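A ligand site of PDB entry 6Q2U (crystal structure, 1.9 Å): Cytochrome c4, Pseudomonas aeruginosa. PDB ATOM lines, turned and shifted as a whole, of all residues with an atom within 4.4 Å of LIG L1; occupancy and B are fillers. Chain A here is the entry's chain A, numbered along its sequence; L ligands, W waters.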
ATOM      1  N   VAL A  13      16.762  -1.502  -6.380  1.00  0.00           N
ATOM      2  CA  VAL A  13      15.358  -1.136  -6.492  1.00  0.00           C
ATOM      3  C   VAL A  13      14.773  -1.630  -7.822  1.00  0.00           C
ATOM      4  O   VAL A  13      13.572  -1.884  -7.920  1.00  0.00           O
ATOM      5  CB  VAL A  13      15.200   0.386  -6.325  1.00  0.00           C
ATOM      6  CG1 VAL A  13      15.854   1.131  -7.481  1.00  0.00           C
ATOM      7  CG2 VAL A  13      13.740   0.780  -6.152  1.00  0.00           C
ATOM      8  N   CYS A  14      15.623  -1.809  -8.839  1.00  0.00           N
ATOM      9  CA  CYS A  14      15.146  -2.266 -10.152  1.00  0.00           C
ATOM     10  C   CYS A  14      14.833  -3.749 -10.187  1.00  0.00           C
ATOM     11  O   CYS A  14      14.054  -4.189 -11.042  1.00  0.00           O
ATOM     12  CB  CYS A  14      16.184  -1.939 -11.233  1.00  0.00           C
ATOM     13  SG  CYS A  14      16.983  -0.310 -11.050  1.00  0.00           S
ATOM     14  N   CYS A  17      11.206  -5.778 -10.467  1.00  0.00           N
ATOM     15  CA  CYS A  17      10.564  -6.086 -11.748  1.00  0.00           C
ATOM     16  C   CYS A  17      11.511  -6.683 -12.764  1.00  0.00           C
ATOM     17  O   CYS A  17      11.089  -7.525 -13.549  1.00  0.00           O
ATOM     18  CB  CYS A  17       9.942  -4.823 -12.358  1.00  0.00           C
ATOM     19  SG  CYS A  17       8.644  -4.113 -11.299  1.00  0.00           S
ATOM     20  N   HIS A  18      12.760  -6.240 -12.802  1.00  0.00           N
ATOM     21  CA  HIS A  18      13.676  -6.658 -13.855  1.00  0.00           C
ATOM     22  C   HIS A  18      14.558  -7.833 -13.447  1.00  0.00           C
ATOM     23  O   HIS A  18      15.330  -8.312 -14.273  1.00  0.00           O
ATOM     24  CB  HIS A  18      14.546  -5.475 -14.299  1.00  0.00           C
ATOM     25  CG  HIS A  18      13.799  -4.403 -15.024  1.00  0.00           C
ATOM     26  ND1 HIS A  18      13.337  -4.540 -16.322  1.00  0.00           N
ATOM     27  CD2 HIS A  18      13.442  -3.155 -14.623  1.00  0.00           C
ATOM     28  CE1 HIS A  18      12.725  -3.415 -16.679  1.00  0.00           C
ATOM     29  NE2 HIS A  18      12.780  -2.569 -15.667  1.00  0.00           N
ATOM     30  N   ASN A  28       6.228  -9.778 -18.781  1.00  0.00           N
ATOM     31  CA  ASN A  28       5.838  -8.396 -19.047  1.00  0.00           C
ATOM     32  C   ASN A  28       6.993  -7.428 -18.878  1.00  0.00           C
ATOM     33  O   ASN A  28       7.002  -6.392 -19.558  1.00  0.00           O
ATOM     34  CB  ASN A  28       4.685  -7.997 -18.118  1.00  0.00           C
ATOM     35  CG  ASN A  28       3.332  -8.383 -18.677  1.00  0.00           C
ATOM     36  OD1 ASN A  28       2.479  -8.905 -17.967  1.00  0.00           O
ATOM     37  ND2 ASN A  28       3.148  -8.154 -19.976  1.00  0.00           N
ATOM     38  N   PHE A  29       7.946  -7.738 -18.035  1.00  0.00           N
ATOM     39  CA  PHE A  29       9.075  -6.863 -17.752  1.00  0.00           C
ATOM     40  C   PHE A  29      10.287  -7.291 -18.548  1.00  0.00           C
ATOM     41  O   PHE A  29      10.667  -8.466 -18.469  1.00  0.00           O
ATOM     42  CB  PHE A  29       9.400  -6.888 -16.272  1.00  0.00           C
ATOM     43  CG  PHE A  29       8.202  -6.610 -15.407  1.00  0.00           C
ATOM     44  CD1 PHE A  29       7.732  -5.316 -15.283  1.00  0.00           C
ATOM     45  CD2 PHE A  29       7.538  -7.632 -14.760  1.00  0.00           C
ATOM     46  CE1 PHE A  29       6.627  -5.038 -14.488  1.00  0.00           C
ATOM     47  CE2 PHE A  29       6.421  -7.361 -13.962  1.00  0.00           C
ATOM     48  CZ  PHE A  29       5.973  -6.063 -13.843  1.00  0.00           C
ATOM     49  N   PRO A  30      10.944  -6.392 -19.277  1.00  0.00           N
ATOM     50  CA  PRO A  30      12.046  -6.832 -20.141  1.00  0.00           C
ATOM     51  C   PRO A  30      13.273  -7.203 -19.318  1.00  0.00           C
ATOM     52  O   PRO A  30      13.561  -6.607 -18.274  1.00  0.00           O
ATOM     53  CB  PRO A  30      12.316  -5.619 -21.039  1.00  0.00           C
ATOM     54  CG  PRO A  30      11.867  -4.437 -20.175  1.00  0.00           C
ATOM     55  CD  PRO A  30      10.669  -4.949 -19.407  1.00  0.00           C
ATOM     56  N   LEU A  32      17.017  -6.886 -18.631  1.00  0.00           N
ATOM     57  CA  LEU A  32      18.048  -5.881 -18.849  1.00  0.00           C
ATOM     58  C   LEU A  32      19.459  -6.474 -18.886  1.00  0.00           C
ATOM     59  O   LEU A  32      20.383  -5.831 -19.384  1.00  0.00           O
ATOM     60  CB  LEU A  32      17.988  -4.810 -17.759  1.00  0.00           C
ATOM     61  CG  LEU A  32      16.635  -4.144 -17.515  1.00  0.00           C
ATOM     62  CD1 LEU A  32      16.752  -3.050 -16.471  1.00  0.00           C
ATOM     63  CD2 LEU A  32      16.090  -3.576 -18.816  1.00  0.00           C
ATOM     64  N   GLN A  35      22.257  -6.344 -21.912  1.00  0.00           N
ATOM     65  CA  GLN A  35      21.919  -5.309 -22.879  1.00  0.00           C
ATOM     66  C   GLN A  35      23.101  -4.335 -23.034  1.00  0.00           C
ATOM     67  O   GLN A  35      23.889  -4.147 -22.101  1.00  0.00           O
ATOM     68  CB  GLN A  35      20.666  -4.579 -22.414  1.00  0.00           C
ATOM     69  CG  GLN A  35      20.093  -3.614 -23.411  1.00  0.00           C
ATOM     70  CD  GLN A  35      19.695  -4.313 -24.682  1.00  0.00           C
ATOM     71  OE1 GLN A  35      20.494  -4.428 -25.611  1.00  0.00           O
ATOM     72  NE2 GLN A  35      18.466  -4.823 -24.725  1.00  0.00           N
ATOM     73  N   TYR A  39      22.719   1.551 -25.149  1.00  0.00           N
ATOM     74  CA  TYR A  39      21.283   1.427 -25.343  1.00  0.00           C
ATOM     75  C   TYR A  39      20.555   1.573 -24.010  1.00  0.00           C
ATOM     76  O   TYR A  39      19.561   2.299 -23.904  1.00  0.00           O
ATOM     77  CB  TYR A  39      20.939   0.084 -25.995  1.00  0.00           C
ATOM     78  CG  TYR A  39      19.440  -0.147 -26.086  1.00  0.00           C
ATOM     79  CD1 TYR A  39      18.690   0.445 -27.103  1.00  0.00           C
ATOM     80  CD2 TYR A  39      18.782  -0.949 -25.160  1.00  0.00           C
ATOM     81  CE1 TYR A  39      17.320   0.256 -27.182  1.00  0.00           C
ATOM     82  CE2 TYR A  39      17.395  -1.132 -25.226  1.00  0.00           C
ATOM     83  CZ  TYR A  39      16.682  -0.519 -26.241  1.00  0.00           C
ATOM     84  OH  TYR A  39      15.327  -0.700 -26.314  1.00  0.00           O
ATOM     85  N   LEU A  40      21.034   0.863 -22.982  1.00  0.00           N
ATOM     86  CA  LEU A  40      20.382   0.956 -21.671  1.00  0.00           C
ATOM     87  C   LEU A  40      20.364   2.390 -21.178  1.00  0.00           C
ATOM     88  O   LEU A  40      19.336   2.882 -20.680  1.00  0.00           O
ATOM     89  CB  LEU A  40      21.107   0.080 -20.660  1.00  0.00           C
ATOM     90  CG  LEU A  40      20.811  -1.418 -20.697  1.00  0.00           C
ATOM     91  CD1 LEU A  40      21.719  -2.145 -19.713  1.00  0.00           C
ATOM     92  CD2 LEU A  40      19.333  -1.711 -20.410  1.00  0.00           C
ATOM     93  N   GLN A  43      17.774   4.539 -23.123  1.00  0.00           N
ATOM     94  CA  GLN A  43      16.409   4.247 -22.674  1.00  0.00           C
ATOM     95  C   GLN A  43      16.117   4.850 -21.299  1.00  0.00           C
ATOM     96  O   GLN A  43      15.020   5.388 -21.076  1.00  0.00           O
ATOM     97  CB  GLN A  43      16.172   2.732 -22.651  1.00  0.00           C
ATOM     98  CG  GLN A  43      16.285   2.081 -24.017  1.00  0.00           C
ATOM     99  CD  GLN A  43      15.381   2.740 -25.049  1.00  0.00           C
ATOM    100  OE1 GLN A  43      14.179   2.897 -24.839  1.00  0.00           O
ATOM    101  NE2 GLN A  43      15.966   3.132 -26.176  1.00  0.00           N
ATOM    102  N   MET A  44      17.073   4.768 -20.371  1.00  0.00           N
ATOM    103  CA  MET A  44      16.875   5.362 -19.044  1.00  0.00           C
ATOM    104  C   MET A  44      16.610   6.859 -19.140  1.00  0.00           C
ATOM    105  O   MET A  44      15.719   7.390 -18.467  1.00  0.00           O
ATOM    106  CB  MET A  44      18.073   5.070 -18.150  1.00  0.00           C
ATOM    107  CG  MET A  44      18.183   3.591 -17.718  1.00  0.00           C
ATOM    108  SD  MET A  44      19.670   3.291 -16.727  1.00  0.00           S
ATOM    109  CE  MET A  44      20.029   1.595 -17.147  1.00  0.00           C
ATOM    110  N   ILE A  47      13.105   7.351 -20.700  1.00  0.00           N
ATOM    111  CA  ILE A  47      12.051   7.110 -19.714  1.00  0.00           C
ATOM    112  C   ILE A  47      12.016   8.239 -18.694  1.00  0.00           C
ATOM    113  O   ILE A  47      10.929   8.719 -18.326  1.00  0.00           O
ATOM    114  CB  ILE A  47      12.246   5.743 -19.041  1.00  0.00           C
ATOM    115  CG1 ILE A  47      12.119   4.593 -20.058  1.00  0.00           C
ATOM    116  CG2 ILE A  47      11.216   5.552 -17.941  1.00  0.00           C
ATOM    117  CD1 ILE A  47      12.566   3.240 -19.519  1.00  0.00           C
ATOM    118  N   ARG A  52       9.999   8.249 -23.739  1.00  0.00           N
ATOM    119  CA  ARG A  52       9.388   6.927 -23.746  1.00  0.00           C
ATOM    120  C   ARG A  52       8.670   6.768 -22.425  1.00  0.00           C
ATOM    121  O   ARG A  52       9.318   6.787 -21.371  1.00  0.00           O
ATOM    122  CB  ARG A  52      10.437   5.826 -23.919  1.00  0.00           C
ATOM    123  CG  ARG A  52       9.842   4.445 -23.864  1.00  0.00           C
ATOM    124  CD  ARG A  52      10.899   3.400 -24.073  1.00  0.00           C
ATOM    125  NE  ARG A  52      10.352   2.070 -23.836  1.00  0.00           N
ATOM    126  CZ  ARG A  52      11.075   0.959 -23.820  1.00  0.00           C
ATOM    127  NH1 ARG A  52      12.378   1.016 -24.024  1.00  0.00           N
ATOM    128  NH2 ARG A  52      10.489  -0.213 -23.566  1.00  0.00           N
ATOM    129  N   VAL A  54       6.926   5.028 -19.475  1.00  0.00           N
ATOM    130  CA  VAL A  54       6.762   3.777 -18.749  1.00  0.00           C
ATOM    131  C   VAL A  54       6.114   4.151 -17.428  1.00  0.00           C
ATOM    132  O   VAL A  54       6.790   4.526 -16.466  1.00  0.00           O
ATOM    133  CB  VAL A  54       8.095   3.037 -18.534  1.00  0.00           C
ATOM    134  CG1 VAL A  54       7.848   1.676 -17.865  1.00  0.00           C
ATOM    135  CG2 VAL A  54       8.823   2.850 -19.863  1.00  0.00           C
ATOM    136  N   GLU A  56       4.702   2.375 -15.207  1.00  0.00           N
ATOM    137  CA  GLU A  56       5.094   1.498 -14.118  1.00  0.00           C
ATOM    138  C   GLU A  56       6.375   1.959 -13.427  1.00  0.00           C
ATOM    139  O   GLU A  56       6.666   1.514 -12.319  1.00  0.00           O
ATOM    140  CB  GLU A  56       5.273   0.061 -14.644  1.00  0.00           C
ATOM    141  CG  GLU A  56       3.985  -0.605 -15.073  1.00  0.00           C
ATOM    142  CD  GLU A  56       3.805  -0.600 -16.592  1.00  0.00           C
ATOM    143  OE1 GLU A  56       4.357   0.301 -17.269  1.00  0.00           O
ATOM    144  OE2 GLU A  56       3.110  -1.507 -17.103  1.00  0.00           O
ATOM    145  N   MET A  57       7.156   2.829 -14.066  1.00  0.00           N
ATOM    146  CA  MET A  57       8.415   3.283 -13.483  1.00  0.00           C
ATOM    147  C   MET A  57       8.337   4.722 -12.988  1.00  0.00           C
ATOM    148  O   MET A  57       9.368   5.290 -12.612  1.00  0.00           O
ATOM    149  CB  MET A  57       9.560   3.135 -14.490  1.00  0.00           C
ATOM    150  CG  MET A  57      10.004   1.686 -14.751  1.00  0.00           C
ATOM    151  SD  MET A  57      11.294   1.554 -16.023  1.00  0.00           S
ATOM    152  CE  MET A  57      12.525   2.650 -15.337  1.00  0.00           C
ATOM    153  N   LEU A  60      10.870   6.492 -10.413  1.00  0.00           N
ATOM    154  CA  LEU A  60      12.014   5.675 -10.022  1.00  0.00           C
ATOM    155  C   LEU A  60      13.347   6.276 -10.466  1.00  0.00           C
ATOM    156  O   LEU A  60      14.350   6.133  -9.768  1.00  0.00           O
ATOM    157  CB  LEU A  60      11.888   4.267 -10.591  1.00  0.00           C
ATOM    158  CG  LEU A  60      10.879   3.360  -9.873  1.00  0.00           C
ATOM    159  CD1 LEU A  60      10.683   2.086 -10.682  1.00  0.00           C
ATOM    160  CD2 LEU A  60      11.347   3.044  -8.451  1.00  0.00           C
ATOM    161  N   LEU A  61      13.378   6.959 -11.605  1.00  0.00           N
ATOM    162  CA  LEU A  61      14.619   7.502 -12.119  1.00  0.00           C
ATOM    163  C   LEU A  61      14.821   8.971 -11.744  1.00  0.00           C
ATOM    164  O   LEU A  61      15.907   9.506 -11.949  1.00  0.00           O
ATOM    165  CB  LEU A  61      14.667   7.345 -13.651  1.00  0.00           C
ATOM    166  CG  LEU A  61      14.460   5.930 -14.193  1.00  0.00           C
ATOM    167  CD1 LEU A  61      14.513   5.940 -15.707  1.00  0.00           C
ATOM    168  CD2 LEU A  61      15.489   4.973 -13.646  1.00  0.00           C
ATOM    169  N   LEU A  64      18.001   9.878  -9.657  1.00  0.00           N
ATOM    170  CA  LEU A  64      19.273   9.251 -10.000  1.00  0.00           C
ATOM    171  C   LEU A  64      20.091  10.233 -10.838  1.00  0.00           C
ATOM    172  O   LEU A  64      19.596  10.775 -11.821  1.00  0.00           O
ATOM    173  CB  LEU A  64      19.046   7.949 -10.761  1.00  0.00           C
ATOM    174  CG  LEU A  64      18.319   6.882  -9.934  1.00  0.00           C
ATOM    175  CD1 LEU A  64      17.990   5.664 -10.803  1.00  0.00           C
ATOM    176  CD2 LEU A  64      19.138   6.476  -8.700  1.00  0.00           C
ATOM    177  N   ILE A  72      24.429   2.006 -13.163  1.00  0.00           N
ATOM    178  CA  ILE A  72      23.392   0.972 -13.279  1.00  0.00           C
ATOM    179  C   ILE A  72      23.451   0.323 -14.656  1.00  0.00           C
ATOM    180  O   ILE A  72      23.407  -0.917 -14.793  1.00  0.00           O
ATOM    181  CB  ILE A  72      22.005   1.568 -13.003  1.00  0.00           C
ATOM    182  CG1 ILE A  72      21.849   1.942 -11.526  1.00  0.00           C
ATOM    183  CG2 ILE A  72      20.903   0.611 -13.479  1.00  0.00           C
ATOM    184  CD1 ILE A  72      20.673   2.850 -11.242  1.00  0.00           C
ATOM    185  N   TYR A 136       7.319  -9.319 -24.289  1.00  0.00           N
ATOM    186  CA  TYR A 136       7.851  -7.951 -24.320  1.00  0.00           C
ATOM    187  C   TYR A 136       8.231  -7.543 -25.735  1.00  0.00           C
ATOM    188  O   TYR A 136       7.907  -6.426 -26.169  1.00  0.00           O
ATOM    189  CB  TYR A 136       9.054  -7.833 -23.374  1.00  0.00           C
ATOM    190  CG  TYR A 136       9.761  -6.512 -23.529  1.00  0.00           C
ATOM    191  CD1 TYR A 136       9.260  -5.358 -22.908  1.00  0.00           C
ATOM    192  CD2 TYR A 136      10.890  -6.392 -24.327  1.00  0.00           C
ATOM    193  CE1 TYR A 136       9.888  -4.133 -23.072  1.00  0.00           C
ATOM    194  CE2 TYR A 136      11.529  -5.159 -24.493  1.00  0.00           C
ATOM    195  CZ  TYR A 136      11.013  -4.031 -23.857  1.00  0.00           C
ATOM    196  OH  TYR A 136      11.631  -2.803 -24.019  1.00  0.00           O
ATOM    197  N   LYS A 139       5.220  -6.706 -27.807  1.00  0.00           N
ATOM    198  CA  LYS A 139       4.670  -5.396 -27.454  1.00  0.00           C
ATOM    199  C   LYS A 139       5.470  -4.270 -28.084  1.00  0.00           C
ATOM    200  O   LYS A 139       4.893  -3.283 -28.561  1.00  0.00           O
ATOM    201  CB  LYS A 139       4.642  -5.244 -25.925  1.00  0.00           C
ATOM    202  CG  LYS A 139       4.220  -3.848 -25.460  1.00  0.00           C
ATOM    203  CD  LYS A 139       4.077  -3.804 -23.942  1.00  0.00           C
ATOM    204  CE  LYS A 139       3.466  -2.485 -23.474  1.00  0.00           C
ATOM    205  NZ  LYS A 139       4.291  -1.315 -23.857  1.00  0.00           N
ATOM    206  N   GLN A 140       6.802  -4.386 -28.108  1.00  0.00           N
ATOM    207  CA  GLN A 140       7.634  -3.349 -28.718  1.00  0.00           C
ATOM    208  C   GLN A 140       7.413  -3.270 -30.223  1.00  0.00           C
ATOM    209  O   GLN A 140       7.229  -2.172 -30.787  1.00  0.00           O
ATOM    210  CB  GLN A 140       9.102  -3.580 -28.393  1.00  0.00           C
ATOM    211  CG  GLN A 140       9.426  -3.549 -26.886  1.00  0.00           C
ATOM    212  CD  GLN A 140       8.728  -2.408 -26.173  1.00  0.00           C
ATOM    213  OE1 GLN A 140       8.985  -1.229 -26.453  1.00  0.00           O
ATOM    214  NE2 GLN A 140       7.838  -2.739 -25.255  1.00  0.00           N
ATOM    215  N   ARG A 149       5.475   3.804 -29.586  1.00  0.00           N
ATOM    216  CA  ARG A 149       6.871   4.011 -29.217  1.00  0.00           C
ATOM    217  C   ARG A 149       7.554   4.772 -30.350  1.00  0.00           C
ATOM    218  O   ARG A 149       7.556   4.309 -31.503  1.00  0.00           O
ATOM    219  CB  ARG A 149       7.599   2.694 -28.921  1.00  0.00           C
ATOM    220  CG  ARG A 149       9.038   2.922 -28.460  1.00  0.00           C
ATOM    221  CD  ARG A 149       9.680   1.688 -27.835  1.00  0.00           C
ATOM    222  NE  ARG A 149      11.140   1.787 -27.880  1.00  0.00           N
ATOM    223  CZ  ARG A 149      11.985   0.822 -27.521  1.00  0.00           C
ATOM    224  NH1 ARG A 149      11.533  -0.339 -27.070  1.00  0.00           N
ATOM    225  NH2 ARG A 149      13.296   1.025 -27.614  1.00  0.00           N
HETATM  226 FE1  LIG L   1      12.129  -0.643 -15.746  1.00  0.00          FE
HETATM  227  C1  LIG L   1      11.495  -0.958 -19.114  1.00  0.00           C
HETATM  228  C2  LIG L   1      15.291   0.424 -16.479  1.00  0.00           C
HETATM  229  C3  LIG L   1      12.808  -0.373 -12.405  1.00  0.00           C
HETATM  230  C4  LIG L   1       9.052  -1.888 -15.028  1.00  0.00           C
HETATM  231  N1  LIG L   1      13.173  -0.342 -17.450  1.00  0.00           N
HETATM  232  C5  LIG L   1      12.756  -0.551 -18.742  1.00  0.00           C
HETATM  233  C6  LIG L   1      13.835  -0.225 -19.657  1.00  0.00           C
HETATM  234  C7  LIG L   1      14.887   0.143 -18.924  1.00  0.00           C
HETATM  235  C8  LIG L   1      14.483   0.081 -17.529  1.00  0.00           C
HETATM  236  C9  LIG L   1      16.296   0.591 -19.362  1.00  0.00           C
HETATM  237  C10 LIG L   1      13.705  -0.379 -21.184  1.00  0.00           C
HETATM  238  C11 LIG L   1      14.352  -1.755 -21.543  1.00  0.00           C
HETATM  239  C12 LIG L   1      14.483  -2.053 -23.040  1.00  0.00           C
HETATM  240  O1  LIG L   1      14.714  -3.256 -23.338  1.00  0.00           O
HETATM  241  O2  LIG L   1      14.200  -1.148 -23.857  1.00  0.00           O
HETATM  242  N2  LIG L   1      13.708  -0.065 -14.684  1.00  0.00           N
HETATM  243  C13 LIG L   1      14.936   0.362 -15.156  1.00  0.00           C
HETATM  244  C14 LIG L   1      15.786   0.709 -14.063  1.00  0.00           C
HETATM  245  C15 LIG L   1      15.083   0.502 -12.936  1.00  0.00           C
HETATM  246  C16 LIG L   1      13.789   0.002 -13.294  1.00  0.00           C
HETATM  247  C17 LIG L   1      17.218   1.233 -14.256  1.00  0.00           C
HETATM  248  C18 LIG L   1      15.564   0.708 -11.462  1.00  0.00           C
HETATM  249  C19 LIG L   1      15.843   2.060 -11.125  1.00  0.00           C
HETATM  250  N3  LIG L   1      11.125  -1.059 -14.052  1.00  0.00           N
HETATM  251  C20 LIG L   1      11.585  -0.914 -12.775  1.00  0.00           C
HETATM  252  C21 LIG L   1      10.555  -1.394 -11.828  1.00  0.00           C
HETATM  253  C22 LIG L   1       9.520  -1.799 -12.582  1.00  0.00           C
HETATM  254  C23 LIG L   1       9.855  -1.615 -13.962  1.00  0.00           C
HETATM  255  C24 LIG L   1      10.768  -1.355 -10.309  1.00  0.00           C
HETATM  256  C25 LIG L   1       8.122  -2.429 -12.164  1.00  0.00           C
HETATM  257  C26 LIG L   1       7.441  -1.774 -11.154  1.00  0.00           C
HETATM  258  N4  LIG L   1      10.584  -1.265 -16.843  1.00  0.00           N
HETATM  259  C27 LIG L   1       9.365  -1.735 -16.370  1.00  0.00           C
HETATM  260  C28 LIG L   1       8.518  -2.055 -17.486  1.00  0.00           C
HETATM  261  C29 LIG L   1       9.188  -1.818 -18.609  1.00  0.00           C
HETATM  262  C30 LIG L   1      10.489  -1.306 -18.232  1.00  0.00           C
HETATM  263  C31 LIG L   1       7.073  -2.616 -17.370  1.00  0.00           C
HETATM  264  C32 LIG L   1       8.714  -2.013 -20.064  1.00  0.00           C
HETATM  265  C33 LIG L   1       7.657  -1.072 -20.625  1.00  0.00           C
HETATM  266  C34 LIG L   1       7.248  -1.352 -22.056  1.00  0.00           C
HETATM  267  O3  LIG L   1       6.544  -2.387 -22.188  1.00  0.00           O
HETATM  268  O4  LIG L   1       7.880  -0.770 -22.971  1.00  0.00           O
HETATM  269 FE1  LG2 L   2      15.256  -3.243 -34.389  1.00  0.00          FE
HETATM  270  C1  LG2 L   2      15.068  -1.588 -31.402  1.00  0.00           C
HETATM  271  C2  LG2 L   2      13.295  -5.720 -33.162  1.00  0.00           C
HETATM  272  C3  LG2 L   2      15.171  -4.691 -37.509  1.00  0.00           C
HETATM  273  C4  LG2 L   2      17.620  -1.069 -35.491  1.00  0.00           C
HETATM  274  N1  LG2 L   2      14.370  -3.586 -32.621  1.00  0.00           N
HETATM  275  C5  LG2 L   2      14.401  -2.792 -31.488  1.00  0.00           C
HETATM  276  C6  LG2 L   2      13.607  -3.433 -30.444  1.00  0.00           C
HETATM  277  C7  LG2 L   2      13.130  -4.581 -30.961  1.00  0.00           C
HETATM  278  C8  LG2 L   2      13.592  -4.684 -32.315  1.00  0.00           C
HETATM  279  C9  LG2 L   2      12.231  -5.682 -30.333  1.00  0.00           C
HETATM  280  C10 LG2 L   2      13.410  -2.858 -29.025  1.00  0.00           C
HETATM  281  C11 LG2 L   2      14.398  -3.555 -28.048  1.00  0.00           C
HETATM  282  C12 LG2 L   2      14.138  -3.299 -26.563  1.00  0.00           C
HETATM  283  O1  LG2 L   2      14.939  -3.867 -25.762  1.00  0.00           O
HETATM  284  O2  LG2 L   2      13.035  -2.766 -26.308  1.00  0.00           O
HETATM  285  N2  LG2 L   2      14.393  -4.866 -35.162  1.00  0.00           N
HETATM  286  C13 LG2 L   2      13.613  -5.785 -34.499  1.00  0.00           C
HETATM  287  C14 LG2 L   2      13.201  -6.811 -35.416  1.00  0.00           C
HETATM  288  C15 LG2 L   2      13.719  -6.496 -36.627  1.00  0.00           C
HETATM  289  C16 LG2 L   2      14.470  -5.294 -36.476  1.00  0.00           C
HETATM  290  C17 LG2 L   2      12.295  -7.998 -34.995  1.00  0.00           C
HETATM  291  C18 LG2 L   2      13.564  -7.286 -37.981  1.00  0.00           C
HETATM  292  C19 LG2 L   2      12.222  -7.419 -38.397  1.00  0.00           C
HETATM  293  N3  LG2 L   2      16.198  -2.942 -36.134  1.00  0.00           N
HETATM  294  C20 LG2 L   2      16.044  -3.659 -37.309  1.00  0.00           C
HETATM  295  C21 LG2 L   2      16.932  -3.135 -38.353  1.00  0.00           C
HETATM  296  C22 LG2 L   2      17.603  -2.122 -37.784  1.00  0.00           C
HETATM  297  C23 LG2 L   2      17.182  -1.996 -36.410  1.00  0.00           C
HETATM  298  C24 LG2 L   2      17.000  -3.711 -39.787  1.00  0.00           C
HETATM  299  C25 LG2 L   2      18.712  -1.224 -38.460  1.00  0.00           C
HETATM  300  C26 LG2 L   2      18.288  -0.481 -39.522  1.00  0.00           C
HETATM  301  N4  LG2 L   2      16.159  -1.638 -33.602  1.00  0.00           N
HETATM  302  C27 LG2 L   2      17.117  -0.863 -34.228  1.00  0.00           C
HETATM  303  C28 LG2 L   2      17.503   0.198 -33.329  1.00  0.00           C
HETATM  304  C29 LG2 L   2      16.802   0.074 -32.198  1.00  0.00           C
HETATM  305  C30 LG2 L   2      15.942  -1.100 -32.349  1.00  0.00           C
HETATM  306  C31 LG2 L   2      18.561   1.244 -33.750  1.00  0.00           C
HETATM  307  C32 LG2 L   2      16.840   0.956 -30.929  1.00  0.00           C
HETATM  308  C33 LG2 L   2      15.765   2.036 -30.811  1.00  0.00           C
HETATM  309  C34 LG2 L   2      15.769   2.874 -29.543  1.00  0.00           C
HETATM  310  O3  LG2 L   2      16.843   3.515 -29.335  1.00  0.00           O
HETATM  311  O4  LG2 L   2      14.694   3.021 -28.908  1.00  0.00           O
HETATM  312  O   HOH W   1       7.550   1.910 -23.619  1.00  0.00           O
HETATM  313  O   HOH W   2      17.084  -4.903 -22.663  1.00  0.00           O
HETATM  314  O   HOH W   3       5.909  -4.799 -21.058  1.00  0.00           O
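An oxygen (O3) of LIG L1 lies within salt-bridge range of the side-chain amino group (NZ) of Lys 139 (3.0 Å). The side-chain hydroxyl of Tyr 39 sits close to an oxygen (O2) of LG2 L2, 3.1 Å away. O4 of LG2 L2 is in hydrogen-bond range of NE2 of Gln 43 (3.0 Å). OH of Tyr 136 lies within hydrogen-bond range of O2 of LIG L1 (3.1 Å). An oxygen (O4) of LG2 L2 lies within salt-bridge range of the guanidinium group (NH2) of Arg 149 (2.8 Å). The side-chain sulfur of Met 57 is bound to an iron atom (FE1) of LIG L1 (2.4 Å). An oxygen (O2) of LIG L1 sits at hydrogen-bond distance from the side-chain hydroxyl (OH) of Tyr 39. An iron atom (FE1) of LIG L1 is bound by a ring nitrogen (NE2) of His 18, 2.0 Å away. The guanidinium group (NH2) of Arg 52 lies within salt-bridge range of an oxygen (O4) of LIG L1. NE2 of Gln 140 is in hydrogen-bond range of O4 of LIG L1, at 3.0 Å. The side-chain sulfur (SG) of Cys 17 is covalently linked to a carbon (C25) of LIG L1, at 2.0 Å. A carbon (C18) of LIG L1 is covalently linked to the side-chain sulfur (SG) of Cys 14 (1.8 Å). O2 of LG2 L2 is in hydrogen-bond range of OH of Tyr 136 (2.7 Å).
An oxygen (O1) of LIG L1 lies close to an oxygen (O1) of LG2 L2.
The guanidinium group of Arg 149 sits at hydrogen-bond distance from the side-chain amide oxygen of Gln 140 (2.8 Å). NH2 of Arg 52 lies within hydrogen-bond range of OE1 of Gln 140, at 3.4 Å. O of Pro 30 sits at hydrogen-bond distance from ND1 of His 18 (2.9 Å). NH2 of Arg 149 lies within hydrogen-bond range of OE1 of Gln 43, 3.5 Å away. NH1 of Arg 52 is in hydrogen-bond range of OE1 of Gln 43 (2.7 Å). The side-chain hydroxyl of Tyr 136 sits at hydrogen-bond distance from the guanidinium group of Arg 52 (2.9 Å). The side-chain hydroxyl (OH) of Tyr 39 is in hydrogen-bond range of the guanidinium group (NH2) of Arg 149 (3.0 Å).
Residues that only touch LIG L1: Val 13 (3.7 Å), Phe 29 (3.5 Å), Pro 30 (3.6 Å), Leu 32 (3.7 Å), Leu 40 (3.95 Å), Gln 43 (3.8 Å), Met 44 (3.9 Å), Ile 47 (3.7 Å), Val 54 (3.8 Å), Glu 56 (3.6 Å), Leu 60 (3.5 Å), Leu 61 (3.9 Å) and Ile 72 (3.8 Å). Hydrophobic or aromatic side chains that line LIG L1: Val 13, His 18, Phe 29, Pro 30, Leu 32, Tyr 39, Leu 40, Met 44, Ile 47, Val 54, Met 57, Leu 60, Leu 61, Ile 72 and Tyr 136. Of the 26 residues printed, 22 come within 4 Å of LIG L1. The nearest printed residue that does not touch LIG L1 is Leu 64 (4.2 Å).
Water W3 lies within hydrogen-bond range of O of Asn 28 (2.4 Å) and O3 of LIG L1 (2.7 Å). Water W1 lies within hydrogen-bond range of O4 of LIG L1 (2.8 Å) and NE of Arg 52 (2.8 Å). Water W2 lies within hydrogen-bond range of NE2 of Gln 35 and O1 of LIG L1.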
